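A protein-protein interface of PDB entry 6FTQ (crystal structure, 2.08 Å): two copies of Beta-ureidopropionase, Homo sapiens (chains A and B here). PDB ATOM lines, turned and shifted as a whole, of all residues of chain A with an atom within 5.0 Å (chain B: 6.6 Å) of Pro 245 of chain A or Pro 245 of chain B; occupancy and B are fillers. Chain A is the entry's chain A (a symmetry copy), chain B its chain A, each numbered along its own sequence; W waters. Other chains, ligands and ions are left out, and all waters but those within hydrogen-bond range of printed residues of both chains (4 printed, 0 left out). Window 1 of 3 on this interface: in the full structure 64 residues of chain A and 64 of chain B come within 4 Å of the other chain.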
ATOM      1  N   HIS A 243      12.657 -19.331 -13.288  1.00  0.00           N
ATOM      2  CA  HIS A 243      12.026 -19.917 -14.488  1.00  0.00           C
ATOM      3  C   HIS A 243      12.768 -21.131 -15.075  1.00  0.00           C
ATOM      4  O   HIS A 243      12.282 -21.738 -16.027  1.00  0.00           O
ATOM      5  CB  HIS A 243      11.851 -18.882 -15.628  1.00  0.00           C
ATOM      6  CG  HIS A 243      11.119 -17.633 -15.243  1.00  0.00           C
ATOM      7  ND1 HIS A 243       9.834 -17.628 -14.729  1.00  0.00           N
ATOM      8  CD2 HIS A 243      11.483 -16.330 -15.349  1.00  0.00           C
ATOM      9  CE1 HIS A 243       9.447 -16.382 -14.517  1.00  0.00           C
ATOM     10  NE2 HIS A 243      10.428 -15.571 -14.890  1.00  0.00           N
ATOM     11  N   HIS A 244      13.936 -21.469 -14.533  1.00  0.00           N
ATOM     12  CA  HIS A 244      14.823 -22.469 -15.081  1.00  0.00           C
ATOM     13  C   HIS A 244      14.993 -23.638 -14.088  1.00  0.00           C
ATOM     14  O   HIS A 244      15.790 -23.535 -13.144  1.00  0.00           O
ATOM     15  CB  HIS A 244      16.167 -21.827 -15.410  1.00  0.00           C
ATOM     16  CG  HIS A 244      16.083 -20.842 -16.528  1.00  0.00           C
ATOM     17  ND1 HIS A 244      16.224 -21.212 -17.849  1.00  0.00           N
ATOM     18  CD2 HIS A 244      15.778 -19.523 -16.532  1.00  0.00           C
ATOM     19  CE1 HIS A 244      16.030 -20.154 -18.620  1.00  0.00           C
ATOM     20  NE2 HIS A 244      15.780 -19.112 -17.844  1.00  0.00           N
ATOM     21  N   PRO A 245      14.242 -24.749 -14.300  1.00  0.00           N
ATOM     22  CA  PRO A 245      14.355 -25.949 -13.449  1.00  0.00           C
ATOM     23  C   PRO A 245      15.795 -26.437 -13.267  1.00  0.00           C
ATOM     24  O   PRO A 245      16.146 -26.894 -12.188  1.00  0.00           O
ATOM     25  CB  PRO A 245      13.517 -26.995 -14.191  1.00  0.00           C
ATOM     26  CG  PRO A 245      12.473 -26.189 -14.910  1.00  0.00           C
ATOM     27  CD  PRO A 245      13.146 -24.879 -15.277  1.00  0.00           C
ATOM     28  N   LEU A 246      16.615 -26.329 -14.309  1.00  0.00           N
ATOM     29  CA  LEU A 246      18.024 -26.710 -14.206  1.00  0.00           C
ATOM     30  C   LEU A 246      18.837 -25.879 -13.180  1.00  0.00           C
ATOM     31  O   LEU A 246      19.757 -26.405 -12.556  1.00  0.00           O
ATOM     32  CB  LEU A 246      18.705 -26.684 -15.568  1.00  0.00           C
ATOM     33  CG  LEU A 246      18.486 -27.916 -16.430  1.00  0.00           C
ATOM     34  CD1 LEU A 246      18.974 -27.679 -17.847  1.00  0.00           C
ATOM     35  CD2 LEU A 246      19.207 -29.103 -15.827  1.00  0.00           C
ATOM     36  N   ASN A 247      18.483 -24.607 -13.017  1.00  0.00           N
ATOM     37  CA  ASN A 247      19.165 -23.716 -12.066  1.00  0.00           C
ATOM     38  C   ASN A 247      18.891 -24.204 -10.642  1.00  0.00           C
ATOM     39  O   ASN A 247      19.829 -24.445  -9.877  1.00  0.00           O
ATOM     40  CB  ASN A 247      18.706 -22.264 -12.286  1.00  0.00           C
ATOM     41  CG  ASN A 247      19.626 -21.226 -11.651  1.00  0.00           C
ATOM     42  OD1 ASN A 247      20.850 -21.376 -11.620  1.00  0.00           O
ATOM     43  ND2 ASN A 247      19.030 -20.118 -11.203  1.00  0.00           N
ATOM     44  N   TRP A 248      17.616 -24.413 -10.316  1.00  0.00           N
ATOM     45  CA  TRP A 248      17.235 -25.003  -9.028  1.00  0.00           C
ATOM     46  C   TRP A 248      17.921 -26.356  -8.811  1.00  0.00           C
ATOM     47  O   TRP A 248      18.494 -26.590  -7.749  1.00  0.00           O
ATOM     48  CB  TRP A 248      15.729 -25.249  -8.933  1.00  0.00           C
ATOM     49  CG  TRP A 248      14.819 -24.061  -9.045  1.00  0.00           C
ATOM     50  CD1 TRP A 248      14.154 -23.648 -10.166  1.00  0.00           C
ATOM     51  CD2 TRP A 248      14.406 -23.190  -7.992  1.00  0.00           C
ATOM     52  NE1 TRP A 248      13.379 -22.564  -9.887  1.00  0.00           N
ATOM     53  CE2 TRP A 248      13.497 -22.263  -8.554  1.00  0.00           C
ATOM     54  CE3 TRP A 248      14.712 -23.098  -6.633  1.00  0.00           C
ATOM     55  CZ2 TRP A 248      12.888 -21.267  -7.804  1.00  0.00           C
ATOM     56  CZ3 TRP A 248      14.112 -22.100  -5.879  1.00  0.00           C
ATOM     57  CH2 TRP A 248      13.198 -21.201  -6.469  1.00  0.00           C
ATOM     58  N   LEU A 249      17.877 -27.221  -9.826  1.00  0.00           N
ATOM     59  CA  LEU A 249      18.497 -28.556  -9.752  1.00  0.00           C
ATOM     60  C   LEU A 249      19.972 -28.521  -9.349  1.00  0.00           C
ATOM     61  O   LEU A 249      20.380 -29.233  -8.451  1.00  0.00           O
ATOM     62  CB  LEU A 249      18.332 -29.334 -11.078  1.00  0.00           C
ATOM     63  CG  LEU A 249      19.076 -30.669 -11.197  1.00  0.00           C
ATOM     64  CD1 LEU A 249      18.592 -31.637 -10.132  1.00  0.00           C
ATOM     65  CD2 LEU A 249      18.891 -31.279 -12.576  1.00  0.00           C
ATOM     66  N   ASN A 280       7.087 -25.847  -7.302  1.00  0.00           N
ATOM     67  CA  ASN A 280       7.510 -27.059  -7.994  1.00  0.00           C
ATOM     68  C   ASN A 280       8.978 -27.388  -7.726  1.00  0.00           C
ATOM     69  O   ASN A 280       9.342 -28.579  -7.602  1.00  0.00           O
ATOM     70  CB  ASN A 280       7.273 -26.943  -9.487  1.00  0.00           C
ATOM     71  CG  ASN A 280       7.519 -28.245 -10.206  1.00  0.00           C
ATOM     72  OD1 ASN A 280       8.510 -28.375 -10.931  1.00  0.00           O
ATOM     73  ND2 ASN A 280       6.662 -29.219  -9.988  1.00  0.00           N
ATOM     74  N   ALA A 284      10.438 -31.061  -6.704  1.00  0.00           N
ATOM     75  CA  ALA A 284      11.359 -31.757  -7.601  1.00  0.00           C
ATOM     76  C   ALA A 284      12.723 -32.033  -6.959  1.00  0.00           C
ATOM     77  O   ALA A 284      13.343 -33.033  -7.259  1.00  0.00           O
ATOM     78  CB  ALA A 284      11.554 -30.960  -8.898  1.00  0.00           C
ATOM     79  N   GLY B 241       7.642 -40.371 -14.447  1.00  0.00           N
ATOM     80  CA  GLY B 241       8.443 -39.382 -15.167  1.00  0.00           C
ATOM     81  C   GLY B 241       7.983 -37.942 -15.051  1.00  0.00           C
ATOM     82  O   GLY B 241       8.767 -37.025 -15.283  1.00  0.00           O
ATOM     83  N   ARG B 242       6.717 -37.737 -14.693  1.00  0.00           N
ATOM     84  CA  ARG B 242       6.210 -36.408 -14.394  1.00  0.00           C
ATOM     85  C   ARG B 242       6.985 -35.706 -13.258  1.00  0.00           C
ATOM     86  O   ARG B 242       7.012 -34.472 -13.239  1.00  0.00           O
ATOM     87  CB  ARG B 242       4.710 -36.450 -14.069  1.00  0.00           C
ATOM     88  CG  ARG B 242       4.356 -37.077 -12.718  1.00  0.00           C
ATOM     89  CD  ARG B 242       2.849 -37.283 -12.594  1.00  0.00           C
ATOM     90  NE  ARG B 242       2.516 -37.814 -11.278  1.00  0.00           N
ATOM     91  CZ  ARG B 242       2.478 -39.105 -10.950  1.00  0.00           C
ATOM     92  NH1 ARG B 242       2.205 -39.445  -9.696  1.00  0.00           N
ATOM     93  NH2 ARG B 242       2.708 -40.074 -11.847  1.00  0.00           N
ATOM     94  N   HIS B 243       7.624 -36.480 -12.363  1.00  0.00           N
ATOM     95  CA  HIS B 243       8.397 -35.939 -11.227  1.00  0.00           C
ATOM     96  C   HIS B 243       9.792 -35.404 -11.599  1.00  0.00           C
ATOM     97  O   HIS B 243      10.483 -34.862 -10.739  1.00  0.00           O
ATOM     98  CB  HIS B 243       8.584 -36.978 -10.093  1.00  0.00           C
ATOM     99  CG  HIS B 243       7.316 -37.592  -9.581  1.00  0.00           C
ATOM    100  ND1 HIS B 243       6.270 -36.856  -9.050  1.00  0.00           N
ATOM    101  CD2 HIS B 243       6.949 -38.893  -9.473  1.00  0.00           C
ATOM    102  CE1 HIS B 243       5.309 -37.674  -8.658  1.00  0.00           C
ATOM    103  NE2 HIS B 243       5.697 -38.920  -8.898  1.00  0.00           N
ATOM    104  N   HIS B 244      10.210 -35.570 -12.852  1.00  0.00           N
ATOM    105  CA  HIS B 244      11.550 -35.278 -13.303  1.00  0.00           C
ATOM    106  C   HIS B 244      11.528 -34.156 -14.362  1.00  0.00           C
ATOM    107  O   HIS B 244      11.255 -34.425 -15.541  1.00  0.00           O
ATOM    108  CB  HIS B 244      12.185 -36.548 -13.861  1.00  0.00           C
ATOM    109  CG  HIS B 244      12.429 -37.584 -12.815  1.00  0.00           C
ATOM    110  ND1 HIS B 244      13.594 -37.629 -12.079  1.00  0.00           N
ATOM    111  CD2 HIS B 244      11.625 -38.551 -12.313  1.00  0.00           C
ATOM    112  CE1 HIS B 244      13.506 -38.597 -11.181  1.00  0.00           C
ATOM    113  NE2 HIS B 244      12.328 -39.186 -11.318  1.00  0.00           N
ATOM    114  N   PRO B 245      11.814 -32.897 -13.941  1.00  0.00           N
ATOM    115  CA  PRO B 245      11.874 -31.752 -14.870  1.00  0.00           C
ATOM    116  C   PRO B 245      12.759 -32.003 -16.094  1.00  0.00           C
ATOM    117  O   PRO B 245      12.427 -31.552 -17.182  1.00  0.00           O
ATOM    118  CB  PRO B 245      12.447 -30.621 -14.009  1.00  0.00           C
ATOM    119  CG  PRO B 245      11.989 -30.950 -12.616  1.00  0.00           C
ATOM    120  CD  PRO B 245      11.963 -32.466 -12.540  1.00  0.00           C
ATOM    121  N   LEU B 246      13.864 -32.721 -15.915  1.00  0.00           N
ATOM    122  CA  LEU B 246      14.733 -33.065 -17.041  1.00  0.00           C
ATOM    123  C   LEU B 246      14.058 -33.939 -18.128  1.00  0.00           C
ATOM    124  O   LEU B 246      14.377 -33.808 -19.308  1.00  0.00           O
ATOM    125  CB  LEU B 246      16.024 -33.717 -16.563  1.00  0.00           C
ATOM    126  CG  LEU B 246      17.102 -32.758 -16.085  1.00  0.00           C
ATOM    127  CD1 LEU B 246      18.224 -33.507 -15.391  1.00  0.00           C
ATOM    128  CD2 LEU B 246      17.652 -31.975 -17.259  1.00  0.00           C
ATOM    129  N   ASN B 247      13.135 -34.806 -17.719  1.00  0.00           N
ATOM    130  CA  ASN B 247      12.411 -35.683 -18.650  1.00  0.00           C
ATOM    131  C   ASN B 247      11.521 -34.826 -19.553  1.00  0.00           C
ATOM    132  O   ASN B 247      11.615 -34.913 -20.780  1.00  0.00           O
ATOM    133  CB  ASN B 247      11.607 -36.735 -17.864  1.00  0.00           C
ATOM    134  CG  ASN B 247      11.156 -37.922 -18.710  1.00  0.00           C
ATOM    135  OD1 ASN B 247      11.865 -38.385 -19.607  1.00  0.00           O
ATOM    136  ND2 ASN B 247       9.988 -38.469 -18.366  1.00  0.00           N
ATOM    137  N   TRP B 248      10.715 -33.956 -18.946  1.00  0.00           N
ATOM    138  CA  TRP B 248       9.911 -32.989 -19.703  1.00  0.00           C
ATOM    139  C   TRP B 248      10.790 -32.134 -20.621  1.00  0.00           C
ATOM    140  O   TRP B 248      10.480 -31.983 -21.801  1.00  0.00           O
ATOM    141  CB  TRP B 248       9.159 -32.026 -18.784  1.00  0.00           C
ATOM    142  CG  TRP B 248       8.168 -32.610 -17.820  1.00  0.00           C
ATOM    143  CD1 TRP B 248       8.382 -32.880 -16.497  1.00  0.00           C
ATOM    144  CD2 TRP B 248       6.797 -32.914 -18.073  1.00  0.00           C
ATOM    145  NE1 TRP B 248       7.245 -33.356 -15.919  1.00  0.00           N
ATOM    146  CE2 TRP B 248       6.244 -33.376 -16.855  1.00  0.00           C
ATOM    147  CE3 TRP B 248       5.979 -32.843 -19.203  1.00  0.00           C
ATOM    148  CZ2 TRP B 248       4.914 -33.757 -16.737  1.00  0.00           C
ATOM    149  CZ3 TRP B 248       4.651 -33.229 -19.092  1.00  0.00           C
ATOM    150  CH2 TRP B 248       4.129 -33.672 -17.859  1.00  0.00           C
ATOM    151  N   LEU B 249      11.888 -31.603 -20.078  1.00  0.00           N
ATOM    152  CA  LEU B 249      12.821 -30.762 -20.849  1.00  0.00           C
ATOM    153  C   LEU B 249      13.316 -31.423 -22.136  1.00  0.00           C
ATOM    154  O   LEU B 249      13.264 -30.824 -23.193  1.00  0.00           O
ATOM    155  CB  LEU B 249      14.025 -30.314 -19.989  1.00  0.00           C
ATOM    156  CG  LEU B 249      15.157 -29.574 -20.711  1.00  0.00           C
ATOM    157  CD1 LEU B 249      14.637 -28.288 -21.326  1.00  0.00           C
ATOM    158  CD2 LEU B 249      16.306 -29.271 -19.764  1.00  0.00           C
ATOM    159  N   MET B 250      13.794 -32.653 -22.050  1.00  0.00           N
ATOM    160  CA  MET B 250      14.355 -33.309 -23.235  1.00  0.00           C
ATOM    161  C   MET B 250      13.335 -33.539 -24.331  1.00  0.00           C
ATOM    162  O   MET B 250      13.663 -33.380 -25.500  1.00  0.00           O
ATOM    163  CB  MET B 250      15.076 -34.611 -22.878  1.00  0.00           C
ATOM    164  CG  MET B 250      16.361 -34.387 -22.104  1.00  0.00           C
ATOM    165  SD  MET B 250      17.498 -33.166 -22.821  1.00  0.00           S
ATOM    166  CE  MET B 250      17.656 -33.774 -24.487  1.00  0.00           C
ATOM    167  N   GLU B 277       3.072 -30.336 -10.868  1.00  0.00           N
ATOM    168  CA  GLU B 277       4.198 -30.804 -11.681  1.00  0.00           C
ATOM    169  C   GLU B 277       3.988 -30.664 -13.172  1.00  0.00           C
ATOM    170  O   GLU B 277       4.823 -30.060 -13.846  1.00  0.00           O
ATOM    171  CB  GLU B 277       4.610 -32.229 -11.283  1.00  0.00           C
ATOM    172  CG  GLU B 277       5.145 -32.269  -9.861  1.00  0.00           C
ATOM    173  CD  GLU B 277       5.715 -33.626  -9.462  1.00  0.00           C
ATOM    174  OE1 GLU B 277       6.922 -33.697  -9.148  1.00  0.00           O
ATOM    175  OE2 GLU B 277       4.958 -34.617  -9.489  1.00  0.00           O
ATOM    176  N   ASN B 280       3.694 -26.945 -14.090  1.00  0.00           N
ATOM    177  CA  ASN B 280       4.989 -26.279 -14.168  1.00  0.00           C
ATOM    178  C   ASN B 280       5.752 -26.660 -15.436  1.00  0.00           C
ATOM    179  O   ASN B 280       6.443 -25.804 -16.034  1.00  0.00           O
ATOM    180  CB  ASN B 280       5.833 -26.589 -12.948  1.00  0.00           C
ATOM    181  CG  ASN B 280       7.096 -25.766 -12.905  1.00  0.00           C
ATOM    182  OD1 ASN B 280       8.190 -26.298 -13.115  1.00  0.00           O
ATOM    183  ND2 ASN B 280       6.962 -24.477 -12.679  1.00  0.00           N
ATOM    184  N   ALA B 281       5.622 -27.926 -15.857  1.00  0.00           N
ATOM    185  CA  ALA B 281       6.330 -28.380 -17.046  1.00  0.00           C
ATOM    186  C   ALA B 281       5.876 -27.657 -18.328  1.00  0.00           C
ATOM    187  O   ALA B 281       6.704 -27.360 -19.187  1.00  0.00           O
ATOM    188  CB  ALA B 281       6.227 -29.881 -17.202  1.00  0.00           C
ATOM    189  N   ALA B 284       7.624 -24.045 -17.953  1.00  0.00           N
ATOM    190  CA  ALA B 284       9.075 -24.102 -18.119  1.00  0.00           C
ATOM    191  C   ALA B 284       9.498 -24.394 -19.563  1.00  0.00           C
ATOM    192  O   ALA B 284      10.525 -23.918 -20.002  1.00  0.00           O
ATOM    193  CB  ALA B 284       9.684 -25.155 -17.183  1.00  0.00           C
ATOM    194  N   ASN B 285       8.708 -25.180 -20.270  1.00  0.00           N
ATOM    195  CA  ASN B 285       9.049 -25.631 -21.606  1.00  0.00           C
ATOM    196  C   ASN B 285       8.261 -24.941 -22.722  1.00  0.00           C
ATOM    197  O   ASN B 285       8.402 -25.295 -23.892  1.00  0.00           O
ATOM    198  CB  ASN B 285       8.872 -27.153 -21.669  1.00  0.00           C
ATOM    199  CG  ASN B 285       9.830 -27.865 -20.731  1.00  0.00           C
ATOM    200  OD1 ASN B 285      11.038 -27.861 -20.962  1.00  0.00           O
ATOM    201  ND2 ASN B 285       9.317 -28.407 -19.649  1.00  0.00           N
ATOM    202  N   TYR B 371      24.869 -26.187 -18.485  1.00  0.00           N
ATOM    203  CA  TYR B 371      24.320 -27.265 -17.655  1.00  0.00           C
ATOM    204  C   TYR B 371      24.821 -28.661 -18.041  1.00  0.00           C
ATOM    205  O   TYR B 371      25.052 -29.488 -17.165  1.00  0.00           O
ATOM    206  CB  TYR B 371      22.782 -27.214 -17.604  1.00  0.00           C
ATOM    207  CG  TYR B 371      22.323 -26.052 -16.753  1.00  0.00           C
ATOM    208  CD1 TYR B 371      22.459 -26.096 -15.364  1.00  0.00           C
ATOM    209  CD2 TYR B 371      21.813 -24.888 -17.331  1.00  0.00           C
ATOM    210  CE1 TYR B 371      22.067 -25.030 -14.567  1.00  0.00           C
ATOM    211  CE2 TYR B 371      21.425 -23.810 -16.543  1.00  0.00           C
ATOM    212  CZ  TYR B 371      21.566 -23.877 -15.158  1.00  0.00           C
ATOM    213  OH  TYR B 371      21.182 -22.823 -14.355  1.00  0.00           O
HETATM  214  O   HOH W   1       8.619 -31.913 -10.074  1.00  0.00           O
HETATM  215  O   HOH W   2      12.575 -23.083 -18.442  1.00  0.00           O
HETATM  216  O   HOH W   3      12.961 -34.397  -9.566  1.00  0.00           O
HETATM  217  O   HOH W   4       7.586 -30.041 -13.628  1.00  0.00           O
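The side-chain amide oxygen (OD1) of Asn 280 of chain A lies close to the side-chain amide oxygen (OD1) of Asn 280 of chain B.
The side-chain hydroxyl (OH) of Tyr 371 of chain B lies within hydrogen-bond range of the side-chain amide oxygen (OD1) of Asn 247 of chain A (3.1 Å).
A ring nitrogen (ND1) of His 243 of chain B is in hydrogen-bond range of the side-chain carboxylate (OE2) of Glu 277 of chain B (2.6 Å).
Among the printed residues, merely in contact across the chains: Pro 245 of chain A with Pro 245 of chain B (3.8 Å), Pro 245 of chain A with Ala 284 of chain B (3.7 Å), Leu 246 of chain A with Leu 246 of chain B (3.6 Å), Leu 246 of chain A with Leu 249 of chain B (3.7 Å), Leu 246 of chain A with Tyr 371 of chain B (3.4 Å), Leu 249 of chain A with Leu 246 of chain B (3.7 Å), Asn 280 of chain A with Glu 277 of chain B (3.4 Å) and Ala 284 of chain A with Pro 245 of chain B (3.7 Å).
Pro 245 of chain A touches just these residues of chain B: Pro 245 and Ala 284.
Pro 245 of chain B touches just these residues of chain A: Pro 245 (3.8 Å) and Ala 284 (3.7 Å).
Of the printed residues of chain B, Asn 280 of chain A touches Glu 277 (3.4 Å) and Asn 280 (3.0 Å).
Printed residues of chain A within 4 Å of Tyr 371 of chain B: Leu 246 (3.4 Å) and Asn 247 (3.1 Å).
Printed residues of chain A within 4 Å of Ala 284 of chain B: Pro 245 (3.7 Å).
The nearest residue of chain A that does not touch Pro 245 of chain B is Asn 280 of chain A (4.6 Å).
Among the printed residues, 10 pairs touch across the chains.
Pro 245 of chain B touches its own counterpart, Pro 245 of chain A.
Pro 245 of chain A touches Ala 284 of chain B, and with the chains exchanged Ala 284 of chain A touches Pro 245 of chain B.
Leu 246 of chain A touches Leu 249 of chain B, and with the chains exchanged Leu 249 of chain A touches Leu 246 of chain B.
Asn 280 of chain A touches its own counterpart, Asn 280 of chain B.
9 positions are printed for both chains.
Water W1 lies within hydrogen-bond range of the side-chain carboxylate (OE1) of Glu 277 of chain B and the side-chain amide nitrogen (ND2) of Asn 280 of chain A.
Water W2 bridges O of Ala 284 of chain B and O of His 243 of chain A.
Water W3 lies within hydrogen-bond range of O of Ala 284 of chain A and O of His 243 of chain B.
Water W4 lies within hydrogen-bond range of the backbone carbonyl oxygen (O) of Glu 277 of chain B (2.8 Å) and the side-chain amide oxygen (OD1) of Asn 280 of chain A (3.3 Å).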
